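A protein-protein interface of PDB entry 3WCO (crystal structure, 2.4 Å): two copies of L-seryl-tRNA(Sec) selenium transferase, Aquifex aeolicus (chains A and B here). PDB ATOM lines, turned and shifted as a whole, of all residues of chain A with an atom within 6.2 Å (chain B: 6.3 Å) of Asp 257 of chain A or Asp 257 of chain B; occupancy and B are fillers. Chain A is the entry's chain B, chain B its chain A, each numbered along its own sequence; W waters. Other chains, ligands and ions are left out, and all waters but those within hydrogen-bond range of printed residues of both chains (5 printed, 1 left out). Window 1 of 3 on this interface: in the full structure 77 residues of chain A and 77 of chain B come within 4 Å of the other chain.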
ATOM      1  N   LEU A  47     -18.249 -30.592 -29.748  1.00  0.00           N
ATOM      2  CA  LEU A  47     -18.529 -29.300 -30.395  1.00  0.00           C
ATOM      3  C   LEU A  47     -17.398 -28.790 -31.285  1.00  0.00           C
ATOM      4  O   LEU A  47     -17.620 -28.384 -32.415  1.00  0.00           O
ATOM      5  CB  LEU A  47     -18.860 -28.239 -29.334  1.00  0.00           C
ATOM      6  CG  LEU A  47     -19.043 -26.817 -29.856  1.00  0.00           C
ATOM      7  CD1 LEU A  47     -20.253 -26.751 -30.746  1.00  0.00           C
ATOM      8  CD2 LEU A  47     -19.158 -25.809 -28.726  1.00  0.00           C
ATOM      9  N   ARG A  59     -16.442 -26.208 -35.537  1.00  0.00           N
ATOM     10  CA  ARG A  59     -17.824 -26.598 -35.286  1.00  0.00           C
ATOM     11  C   ARG A  59     -18.704 -26.621 -36.549  1.00  0.00           C
ATOM     12  O   ARG A  59     -19.697 -27.347 -36.611  1.00  0.00           O
ATOM     13  CB  ARG A  59     -18.427 -25.684 -34.220  1.00  0.00           C
ATOM     14  CG  ARG A  59     -18.518 -24.229 -34.632  1.00  0.00           C
ATOM     15  CD  ARG A  59     -18.916 -23.354 -33.441  1.00  0.00           C
ATOM     16  NE  ARG A  59     -17.867 -23.281 -32.416  1.00  0.00           N
ATOM     17  CZ  ARG A  59     -18.060 -22.804 -31.194  1.00  0.00           C
ATOM     18  NH1 ARG A  59     -19.263 -22.371 -30.836  1.00  0.00           N
ATOM     19  NH2 ARG A  59     -17.058 -22.770 -30.331  1.00  0.00           N
ATOM     20  N   ASN A  80     -23.650 -15.935 -36.355  1.00  0.00           N
ATOM     21  CA  ASN A  80     -24.594 -15.605 -35.293  1.00  0.00           C
ATOM     22  C   ASN A  80     -26.006 -15.319 -35.781  1.00  0.00           C
ATOM     23  O   ASN A  80     -26.961 -15.909 -35.293  1.00  0.00           O
ATOM     24  CB  ASN A  80     -24.084 -14.409 -34.499  1.00  0.00           C
ATOM     25  CG  ASN A  80     -25.077 -13.952 -33.472  1.00  0.00           C
ATOM     26  OD1 ASN A  80     -25.583 -14.756 -32.670  1.00  0.00           O
ATOM     27  ND2 ASN A  80     -25.382 -12.654 -33.490  1.00  0.00           N
ATOM     28  N   PRO A 230     -33.335 -22.413 -34.996  1.00  0.00           N
ATOM     29  CA  PRO A 230     -32.999 -21.287 -34.115  1.00  0.00           C
ATOM     30  C   PRO A 230     -32.347 -20.118 -34.859  1.00  0.00           C
ATOM     31  O   PRO A 230     -32.091 -20.202 -36.074  1.00  0.00           O
ATOM     32  CB  PRO A 230     -32.042 -21.909 -33.104  1.00  0.00           C
ATOM     33  CG  PRO A 230     -31.468 -23.094 -33.794  1.00  0.00           C
ATOM     34  CD  PRO A 230     -32.464 -23.582 -34.788  1.00  0.00           C
ATOM     35  N   GLN A 231     -32.113 -19.015 -34.158  1.00  0.00           N
ATOM     36  CA  GLN A 231     -31.417 -17.876 -34.777  1.00  0.00           C
ATOM     37  C   GLN A 231     -30.068 -18.297 -35.395  1.00  0.00           C
ATOM     38  O   GLN A 231     -29.303 -19.056 -34.791  1.00  0.00           O
ATOM     39  CB  GLN A 231     -31.209 -16.744 -33.763  1.00  0.00           C
ATOM     40  CG  GLN A 231     -30.103 -15.725 -34.137  1.00  0.00           C
ATOM     41  CD  GLN A 231     -29.931 -14.666 -33.072  1.00  0.00           C
ATOM     42  OE1 GLN A 231     -30.924 -14.093 -32.608  1.00  0.00           O
ATOM     43  NE2 GLN A 231     -28.675 -14.409 -32.654  1.00  0.00           N
ATOM     44  N   ARG A 255     -19.119 -16.057 -34.227  1.00  0.00           N
ATOM     45  CA  ARG A 255     -19.210 -17.522 -34.114  1.00  0.00           C
ATOM     46  C   ARG A 255     -20.444 -18.045 -33.391  1.00  0.00           C
ATOM     47  O   ARG A 255     -20.836 -17.546 -32.333  1.00  0.00           O
ATOM     48  CB  ARG A 255     -17.957 -18.108 -33.470  1.00  0.00           C
ATOM     49  CG  ARG A 255     -17.869 -19.637 -33.567  1.00  0.00           C
ATOM     50  CD  ARG A 255     -16.490 -20.121 -33.156  1.00  0.00           C
ATOM     51  NE  ARG A 255     -16.236 -19.930 -31.734  1.00  0.00           N
ATOM     52  CZ  ARG A 255     -15.091 -20.245 -31.139  1.00  0.00           C
ATOM     53  NH1 ARG A 255     -14.105 -20.753 -31.862  1.00  0.00           N
ATOM     54  NH2 ARG A 255     -14.922 -20.047 -29.830  1.00  0.00           N
ATOM     55  N   ILE A 256     -21.044 -19.072 -33.975  1.00  0.00           N
ATOM     56  CA  ILE A 256     -22.303 -19.621 -33.493  1.00  0.00           C
ATOM     57  C   ILE A 256     -22.084 -20.461 -32.249  1.00  0.00           C
ATOM     58  O   ILE A 256     -21.116 -21.220 -32.160  1.00  0.00           O
ATOM     59  CB  ILE A 256     -22.978 -20.476 -34.589  1.00  0.00           C
ATOM     60  CG1 ILE A 256     -23.681 -19.576 -35.596  1.00  0.00           C
ATOM     61  CG2 ILE A 256     -23.989 -21.442 -34.013  1.00  0.00           C
ATOM     62  CD1 ILE A 256     -25.191 -19.785 -35.675  1.00  0.00           C
ATOM     63  N   ASP A 257     -23.006 -20.349 -31.301  1.00  0.00           N
ATOM     64  CA  ASP A 257     -22.877 -21.066 -30.041  1.00  0.00           C
ATOM     65  C   ASP A 257     -23.343 -22.502 -30.208  1.00  0.00           C
ATOM     66  O   ASP A 257     -23.834 -22.881 -31.266  1.00  0.00           O
ATOM     67  CB  ASP A 257     -23.708 -20.387 -28.971  1.00  0.00           C
ATOM     68  CG  ASP A 257     -25.185 -20.413 -29.297  1.00  0.00           C
ATOM     69  OD1 ASP A 257     -25.626 -19.601 -30.143  1.00  0.00           O
ATOM     70  OD2 ASP A 257     -25.910 -21.249 -28.717  1.00  0.00           O
ATOM     71  N   LYS A 258     -23.195 -23.283 -29.141  1.00  0.00           N
ATOM     72  CA  LYS A 258     -23.513 -24.711 -29.131  1.00  0.00           C
ATOM     73  C   LYS A 258     -25.024 -25.022 -29.126  1.00  0.00           C
ATOM     74  O   LYS A 258     -25.463 -26.005 -29.700  1.00  0.00           O
ATOM     75  CB  LYS A 258     -22.788 -25.339 -27.929  1.00  0.00           C
ATOM     76  CG  LYS A 258     -23.368 -26.606 -27.366  1.00  0.00           C
ATOM     77  CD  LYS A 258     -22.464 -27.176 -26.262  1.00  0.00           C
ATOM     78  CE  LYS A 258     -22.063 -26.121 -25.257  1.00  0.00           C
ATOM     79  NZ  LYS A 258     -21.761 -26.711 -23.910  1.00  0.00           N
ATOM     80  N   LEU A 259     -25.819 -24.187 -28.474  1.00  0.00           N
ATOM     81  CA  LEU A 259     -27.250 -24.439 -28.408  1.00  0.00           C
ATOM     82  C   LEU A 259     -27.858 -24.251 -29.796  1.00  0.00           C
ATOM     83  O   LEU A 259     -28.529 -25.136 -30.297  1.00  0.00           O
ATOM     84  CB  LEU A 259     -27.896 -23.498 -27.398  1.00  0.00           C
ATOM     85  CG  LEU A 259     -27.296 -23.600 -25.995  1.00  0.00           C
ATOM     86  CD1 LEU A 259     -27.659 -22.372 -25.120  1.00  0.00           C
ATOM     87  CD2 LEU A 259     -27.754 -24.886 -25.351  1.00  0.00           C
ATOM     88  N   THR A 260     -27.583 -23.117 -30.433  1.00  0.00           N
ATOM     89  CA  THR A 260     -28.114 -22.880 -31.753  1.00  0.00           C
ATOM     90  C   THR A 260     -27.566 -23.860 -32.794  1.00  0.00           C
ATOM     91  O   THR A 260     -28.294 -24.262 -33.729  1.00  0.00           O
ATOM     92  CB  THR A 260     -27.950 -21.399 -32.215  1.00  0.00           C
ATOM     93  OG1 THR A 260     -26.574 -21.045 -32.215  1.00  0.00           O
ATOM     94  CG2 THR A 260     -28.714 -20.449 -31.296  1.00  0.00           C
ATOM     95  N   LEU A 261     -26.305 -24.262 -32.644  1.00  0.00           N
ATOM     96  CA  LEU A 261     -25.721 -25.133 -33.651  1.00  0.00           C
ATOM     97  C   LEU A 261     -26.352 -26.519 -33.577  1.00  0.00           C
ATOM     98  O   LEU A 261     -26.627 -27.138 -34.615  1.00  0.00           O
ATOM     99  CB  LEU A 261     -24.199 -25.238 -33.522  1.00  0.00           C
ATOM    100  CG  LEU A 261     -23.580 -26.168 -34.593  1.00  0.00           C
ATOM    101  CD1 LEU A 261     -23.536 -25.501 -35.944  1.00  0.00           C
ATOM    102  CD2 LEU A 261     -22.204 -26.682 -34.245  1.00  0.00           C
ATOM    103  N   SER A 262     -26.582 -26.995 -32.351  1.00  0.00           N
ATOM    104  CA  SER A 262     -27.196 -28.302 -32.151  1.00  0.00           C
ATOM    105  C   SER A 262     -28.615 -28.251 -32.666  1.00  0.00           C
ATOM    106  O   SER A 262     -29.089 -29.207 -33.278  1.00  0.00           O
ATOM    107  CB  SER A 262     -27.252 -28.631 -30.669  1.00  0.00           C
ATOM    108  OG  SER A 262     -26.001 -28.350 -30.112  1.00  0.00           O
ATOM    109  N   LEU B  47     -39.666 -12.358 -25.739  1.00  0.00           N
ATOM    110  CA  LEU B  47     -38.237 -12.173 -25.972  1.00  0.00           C
ATOM    111  C   LEU B  47     -37.914 -10.733 -26.347  1.00  0.00           C
ATOM    112  O   LEU B  47     -37.011 -10.142 -25.767  1.00  0.00           O
ATOM    113  CB  LEU B  47     -37.738 -13.128 -27.066  1.00  0.00           C
ATOM    114  CG  LEU B  47     -36.298 -12.850 -27.494  1.00  0.00           C
ATOM    115  CD1 LEU B  47     -35.365 -13.226 -26.357  1.00  0.00           C
ATOM    116  CD2 LEU B  47     -35.920 -13.560 -28.794  1.00  0.00           C
ATOM    117  N   ARG B  59     -34.278  -7.178 -25.818  1.00  0.00           N
ATOM    118  CA  ARG B  59     -34.131  -8.392 -25.037  1.00  0.00           C
ATOM    119  C   ARG B  59     -33.172  -8.243 -23.855  1.00  0.00           C
ATOM    120  O   ARG B  59     -33.273  -8.976 -22.868  1.00  0.00           O
ATOM    121  CB  ARG B  59     -33.693  -9.536 -25.958  1.00  0.00           C
ATOM    122  CG  ARG B  59     -32.395  -9.285 -26.707  1.00  0.00           C
ATOM    123  CD  ARG B  59     -32.179 -10.364 -27.767  1.00  0.00           C
ATOM    124  NE  ARG B  59     -32.917 -10.120 -29.007  1.00  0.00           N
ATOM    125  CZ  ARG B  59     -33.124 -11.038 -29.946  1.00  0.00           C
ATOM    126  NH1 ARG B  59     -32.668 -12.278 -29.795  1.00  0.00           N
ATOM    127  NH2 ARG B  59     -33.793 -10.718 -31.041  1.00  0.00           N
ATOM    128  N   ASN B  80     -22.855 -11.737 -28.535  1.00  0.00           N
ATOM    129  CA  ASN B  80     -22.724 -13.115 -28.946  1.00  0.00           C
ATOM    130  C   ASN B  80     -21.671 -13.880 -28.158  1.00  0.00           C
ATOM    131  O   ASN B  80     -21.958 -14.931 -27.581  1.00  0.00           O
ATOM    132  CB  ASN B  80     -22.412 -13.171 -30.441  1.00  0.00           C
ATOM    133  CG  ASN B  80     -22.268 -14.586 -30.953  1.00  0.00           C
ATOM    134  OD1 ASN B  80     -23.080 -15.460 -30.634  1.00  0.00           O
ATOM    135  ND2 ASN B  80     -21.214 -14.829 -31.737  1.00  0.00           N
ATOM    136  N   PRO B 230     -24.232 -20.291 -20.743  1.00  0.00           N
ATOM    137  CA  PRO B 230     -23.923 -20.539 -22.156  1.00  0.00           C
ATOM    138  C   PRO B 230     -23.031 -19.455 -22.746  1.00  0.00           C
ATOM    139  O   PRO B 230     -22.751 -18.462 -22.065  1.00  0.00           O
ATOM    140  CB  PRO B 230     -25.288 -20.475 -22.818  1.00  0.00           C
ATOM    141  CG  PRO B 230     -26.068 -19.561 -21.943  1.00  0.00           C
ATOM    142  CD  PRO B 230     -25.629 -19.866 -20.552  1.00  0.00           C
ATOM    143  N   GLN B 231     -22.567 -19.660 -23.981  1.00  0.00           N
ATOM    144  CA  GLN B 231     -21.753 -18.664 -24.689  1.00  0.00           C
ATOM    145  C   GLN B 231     -22.382 -17.267 -24.656  1.00  0.00           C
ATOM    146  O   GLN B 231     -23.600 -17.113 -24.852  1.00  0.00           O
ATOM    147  CB  GLN B 231     -21.582 -19.085 -26.154  1.00  0.00           C
ATOM    148  CG  GLN B 231     -21.064 -17.999 -27.103  1.00  0.00           C
ATOM    149  CD  GLN B 231     -20.719 -18.571 -28.484  1.00  0.00           C
ATOM    150  OE1 GLN B 231     -20.109 -19.646 -28.579  1.00  0.00           O
ATOM    151  NE2 GLN B 231     -21.121 -17.869 -29.554  1.00  0.00           N
ATOM    152  N   ARG B 255     -25.947  -9.661 -31.987  1.00  0.00           N
ATOM    153  CA  ARG B 255     -27.047  -9.866 -31.042  1.00  0.00           C
ATOM    154  C   ARG B 255     -27.205 -11.312 -30.564  1.00  0.00           C
ATOM    155  O   ARG B 255     -27.138 -12.252 -31.357  1.00  0.00           O
ATOM    156  CB  ARG B 255     -28.370  -9.346 -31.617  1.00  0.00           C
ATOM    157  CG  ARG B 255     -29.470  -9.224 -30.562  1.00  0.00           C
ATOM    158  CD  ARG B 255     -30.661  -8.429 -31.098  1.00  0.00           C
ATOM    159  NE  ARG B 255     -31.360  -9.061 -32.211  1.00  0.00           N
ATOM    160  CZ  ARG B 255     -32.428  -8.533 -32.811  1.00  0.00           C
ATOM    161  NH1 ARG B 255     -32.897  -7.367 -32.399  1.00  0.00           N
ATOM    162  NH2 ARG B 255     -33.029  -9.164 -33.818  1.00  0.00           N
ATOM    163  N   ILE B 256     -27.418 -11.483 -29.263  1.00  0.00           N
ATOM    164  CA  ILE B 256     -27.549 -12.820 -28.698  1.00  0.00           C
ATOM    165  C   ILE B 256     -28.904 -13.389 -28.997  1.00  0.00           C
ATOM    166  O   ILE B 256     -29.902 -12.667 -29.026  1.00  0.00           O
ATOM    167  CB  ILE B 256     -27.414 -12.853 -27.176  1.00  0.00           C
ATOM    168  CG1 ILE B 256     -28.146 -11.654 -26.575  1.00  0.00           C
ATOM    169  CG2 ILE B 256     -25.969 -12.893 -26.783  1.00  0.00           C
ATOM    170  CD1 ILE B 256     -28.487 -11.840 -25.133  1.00  0.00           C
ATOM    171  N   ASP B 257     -28.940 -14.704 -29.161  1.00  0.00           N
ATOM    172  CA  ASP B 257     -30.187 -15.393 -29.442  1.00  0.00           C
ATOM    173  C   ASP B 257     -30.943 -15.740 -28.153  1.00  0.00           C
ATOM    174  O   ASP B 257     -30.425 -15.584 -27.033  1.00  0.00           O
ATOM    175  CB  ASP B 257     -29.898 -16.674 -30.200  1.00  0.00           C
ATOM    176  CG  ASP B 257     -29.160 -17.682 -29.344  1.00  0.00           C
ATOM    177  OD1 ASP B 257     -27.924 -17.545 -29.169  1.00  0.00           O
ATOM    178  OD2 ASP B 257     -29.825 -18.604 -28.829  1.00  0.00           O
ATOM    179  N   LYS B 258     -32.157 -16.238 -28.358  1.00  0.00           N
ATOM    180  CA  LYS B 258     -33.109 -16.640 -27.333  1.00  0.00           C
ATOM    181  C   LYS B 258     -32.617 -17.772 -26.405  1.00  0.00           C
ATOM    182  O   LYS B 258     -32.869 -17.745 -25.201  1.00  0.00           O
ATOM    183  CB  LYS B 258     -34.397 -17.052 -28.076  1.00  0.00           C
ATOM    184  CG  LYS B 258     -35.605 -17.420 -27.244  1.00  0.00           C
ATOM    185  CD  LYS B 258     -36.848 -17.601 -28.139  1.00  0.00           C
ATOM    186  CE  LYS B 258     -36.538 -18.381 -29.393  1.00  0.00           C
ATOM    187  NZ  LYS B 258     -37.744 -19.010 -30.042  1.00  0.00           N
ATOM    188  N   LEU B 259     -31.924 -18.768 -26.954  1.00  0.00           N
ATOM    189  CA  LEU B 259     -31.489 -19.918 -26.142  1.00  0.00           C
ATOM    190  C   LEU B 259     -30.416 -19.481 -25.158  1.00  0.00           C
ATOM    191  O   LEU B 259     -30.514 -19.755 -23.970  1.00  0.00           O
ATOM    192  CB  LEU B 259     -30.968 -21.033 -27.036  1.00  0.00           C
ATOM    193  CG  LEU B 259     -31.934 -21.426 -28.156  1.00  0.00           C
ATOM    194  CD1 LEU B 259     -31.246 -22.325 -29.178  1.00  0.00           C
ATOM    195  CD2 LEU B 259     -33.152 -22.104 -27.564  1.00  0.00           C
ATOM    196  N   THR B 260     -29.421 -18.751 -25.645  1.00  0.00           N
ATOM    197  CA  THR B 260     -28.362 -18.273 -24.770  1.00  0.00           C
ATOM    198  C   THR B 260     -28.860 -17.202 -23.780  1.00  0.00           C
ATOM    199  O   THR B 260     -28.474 -17.196 -22.608  1.00  0.00           O
ATOM    200  CB  THR B 260     -27.093 -17.835 -25.564  1.00  0.00           C
ATOM    201  OG1 THR B 260     -27.375 -16.688 -26.363  1.00  0.00           O
ATOM    202  CG2 THR B 260     -26.605 -18.976 -26.467  1.00  0.00           C
ATOM    203  N   LEU B 261     -29.750 -16.326 -24.226  1.00  0.00           N
ATOM    204  CA  LEU B 261     -30.276 -15.299 -23.340  1.00  0.00           C
ATOM    205  C   LEU B 261     -31.095 -15.900 -22.193  1.00  0.00           C
ATOM    206  O   LEU B 261     -30.946 -15.488 -21.028  1.00  0.00           O
ATOM    207  CB  LEU B 261     -31.109 -14.276 -24.113  1.00  0.00           C
ATOM    208  CG  LEU B 261     -31.778 -13.219 -23.238  1.00  0.00           C
ATOM    209  CD1 LEU B 261     -30.743 -12.517 -22.425  1.00  0.00           C
ATOM    210  CD2 LEU B 261     -32.523 -12.221 -24.069  1.00  0.00           C
ATOM    211  N   SER B 262     -31.936 -16.872 -22.524  1.00  0.00           N
ATOM    212  CA  SER B 262     -32.778 -17.565 -21.564  1.00  0.00           C
ATOM    213  C   SER B 262     -31.890 -18.315 -20.602  1.00  0.00           C
ATOM    214  O   SER B 262     -32.128 -18.321 -19.394  1.00  0.00           O
ATOM    215  CB  SER B 262     -33.634 -18.619 -22.304  1.00  0.00           C
ATOM    216  OG  SER B 262     -34.638 -17.957 -23.021  1.00  0.00           O
HETATM  217  O   HOH W   1     -18.165 -18.629 -30.060  1.00  0.00           O
HETATM  218  O   HOH W   2     -20.827 -22.474 -27.763  1.00  0.00           O
HETATM  219  O   HOH W   3     -33.396 -15.155 -31.084  1.00  0.00           O
HETATM  220  O   HOH W   4     -32.398 -18.980 -31.137  1.00  0.00           O
HETATM  221  O   HOH W   5     -30.456 -11.308 -33.441  1.00  0.00           O
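Of the 13 printed residues of chain B, 9 touch a printed residue of chain A. Hydrophobic or aromatic side chains of chain B within 4 Å of the printed part of chain A: Pro 230 and Leu 259. Hydrophobic or aromatic side chains of chain A within 4 Å of the printed part of chain B: Leu 259. Among the printed residues, no Asp or Glu carboxylate lies within 4 Å of a Lys or Arg side-chain nitrogen of the other chain.
OD1 of Asn 80 of chain B lies close to OD1 of Asn 80 of chain A (3.3 Å). The side-chain amide nitrogen of Asn 80 of chain B is in hydrogen-bond range of the backbone carbonyl oxygen of Arg 255 of chain A, 2.8 Å away. The side-chain amide nitrogen (NE2) of Gln 231 of chain B sits at hydrogen-bond distance from the backbone carbonyl oxygen (O) of Arg 255 of chain A, 2.8 Å away. The side-chain amide nitrogen (ND2) of Asn 80 of chain A lies within hydrogen-bond range of the backbone carbonyl oxygen (O) of Arg 255 of chain B, at 2.8 Å. The backbone carbonyl oxygen (O) of Arg 255 of chain B sits at hydrogen-bond distance from the side-chain amide nitrogen (NE2) of Gln 231 of chain A (2.9 Å). The side-chain carboxylate of Asp 257 of chain A sits close to the side-chain carboxylate of Asp 257 of chain B.
Water W1 lies within hydrogen-bond range of the side-chain amide oxygen of Gln 231 of chain B (2.6 Å) and the guanidinium group of Arg 255 of chain A (2.9 Å). Water W5 bridges the guanidinium group of Arg 255 of chain B and the side-chain amide oxygen of Gln 231 of chain A. Water W2 lies within hydrogen-bond range of the backbone NH of Lys 258 of chain A, the side-chain amide oxygen of Gln 231 of chain B and the guanidinium group of Arg 59 of chain A. Water W4 lies within hydrogen-bond range of the backbone NH of Gln 231 of chain A (3.0 Å) and the side-chain carboxylate of Asp 257 of chain B (3.5 Å). Water W3 lies within hydrogen-bond range of the side-chain amide oxygen of Gln 231 of chain A (3.1 Å), the backbone NH of Lys 258 of chain B (3.2 Å) and the guanidinium group of Arg 59 of chain B (3.2 Å).
The guanidinium group of Arg 59 of chain B sits at hydrogen-bond distance from the backbone carbonyl oxygen of Ile 256 of chain B, 2.9 Å away. The backbone NH (N) of Leu 259 of chain B sits at hydrogen-bond distance from the side-chain carboxylate (OD2) of Asp 257 of chain B. OG1 of Thr 260 of chain B is in hydrogen-bond range of OD1 of Asp 257 of chain B (3.0 Å). OD1 of Asn 80 of chain A is in hydrogen-bond range of NE2 of Gln 231 of chain A (3.1 Å). N of Leu 259 of chain A sits at hydrogen-bond distance from OD2 of Asp 257 of chain A (2.9 Å). The side-chain carboxylate (OD1) of Asp 257 of chain A lies within hydrogen-bond range of the side-chain hydroxyl (OG1) of Thr 260 of chain A, 2.7 Å away.
Asn 80 of chain A touches its own counterpart, Asn 80 of chain B. Asn 80 of chain A touches Arg 255 of chain B, and with the chains exchanged Arg 255 of chain A touches Asn 80 of chain B. Leu 259 of chain A touches its own counterpart, Leu 259 of chain B. Leu 259 of chain A touches Thr 260 of chain B, and with the chains exchanged Thr 260 of chain A touches Leu 259 of chain B.
Of the printed residues of chain B, Arg 59 of chain A touches Gln 231. Of the printed residues of chain B, Asp 257 of chain A touches Gln 231 (3.4 Å), Asp 257 (3.2 Å) and Thr 260 (3.3 Å). Of the printed residues of chain B, Leu 259 of chain A touches Pro 230, Leu 259 and Thr 260. Of the printed residues of chain A, Asn 80 of chain B touches Asn 80 and Arg 255. Printed residues of chain A within 4 Å of Ile 256 of chain B: Gln 231 (3.8 Å). Asp 257 of chain B touches three residues of chain A. Of the printed residues of chain A, Thr 260 of chain B touches Asp 257 and Leu 259. Ser 262 of chain B touches none of the printed residues of chain A. The nearest residue of chain B that does not touch Asp 257 of chain A is Asn 80 of chain B (4.9 Å). The nearest residue of chain A that does not touch Asp 257 of chain B is Asn 80 of chain A (4.9 Å).
Among the printed residues, pairs that only touch across the chains: Asp 257 of chain A with Thr 260 of chain B, Thr 260 of chain A with Asp 257 of chain B, Asp 257 of chain A with Gln 231 of chain B, Gln 231 of chain A with Asp 257 of chain B, Arg 59 of chain A with Gln 231 of chain B, Gln 231 of chain A with Arg 59 of chain B, Thr 260 of chain A with Leu 259 of chain B, Leu 259 of chain A with Thr 260 of chain B, Gln 231 of chain A with Ile 256 of chain B, Leu 259 of chain A with Pro 230 of chain B, Ile 256 of chain A with Gln 231 of chain B and Leu 259 of chain A with Leu 259 of chain B.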
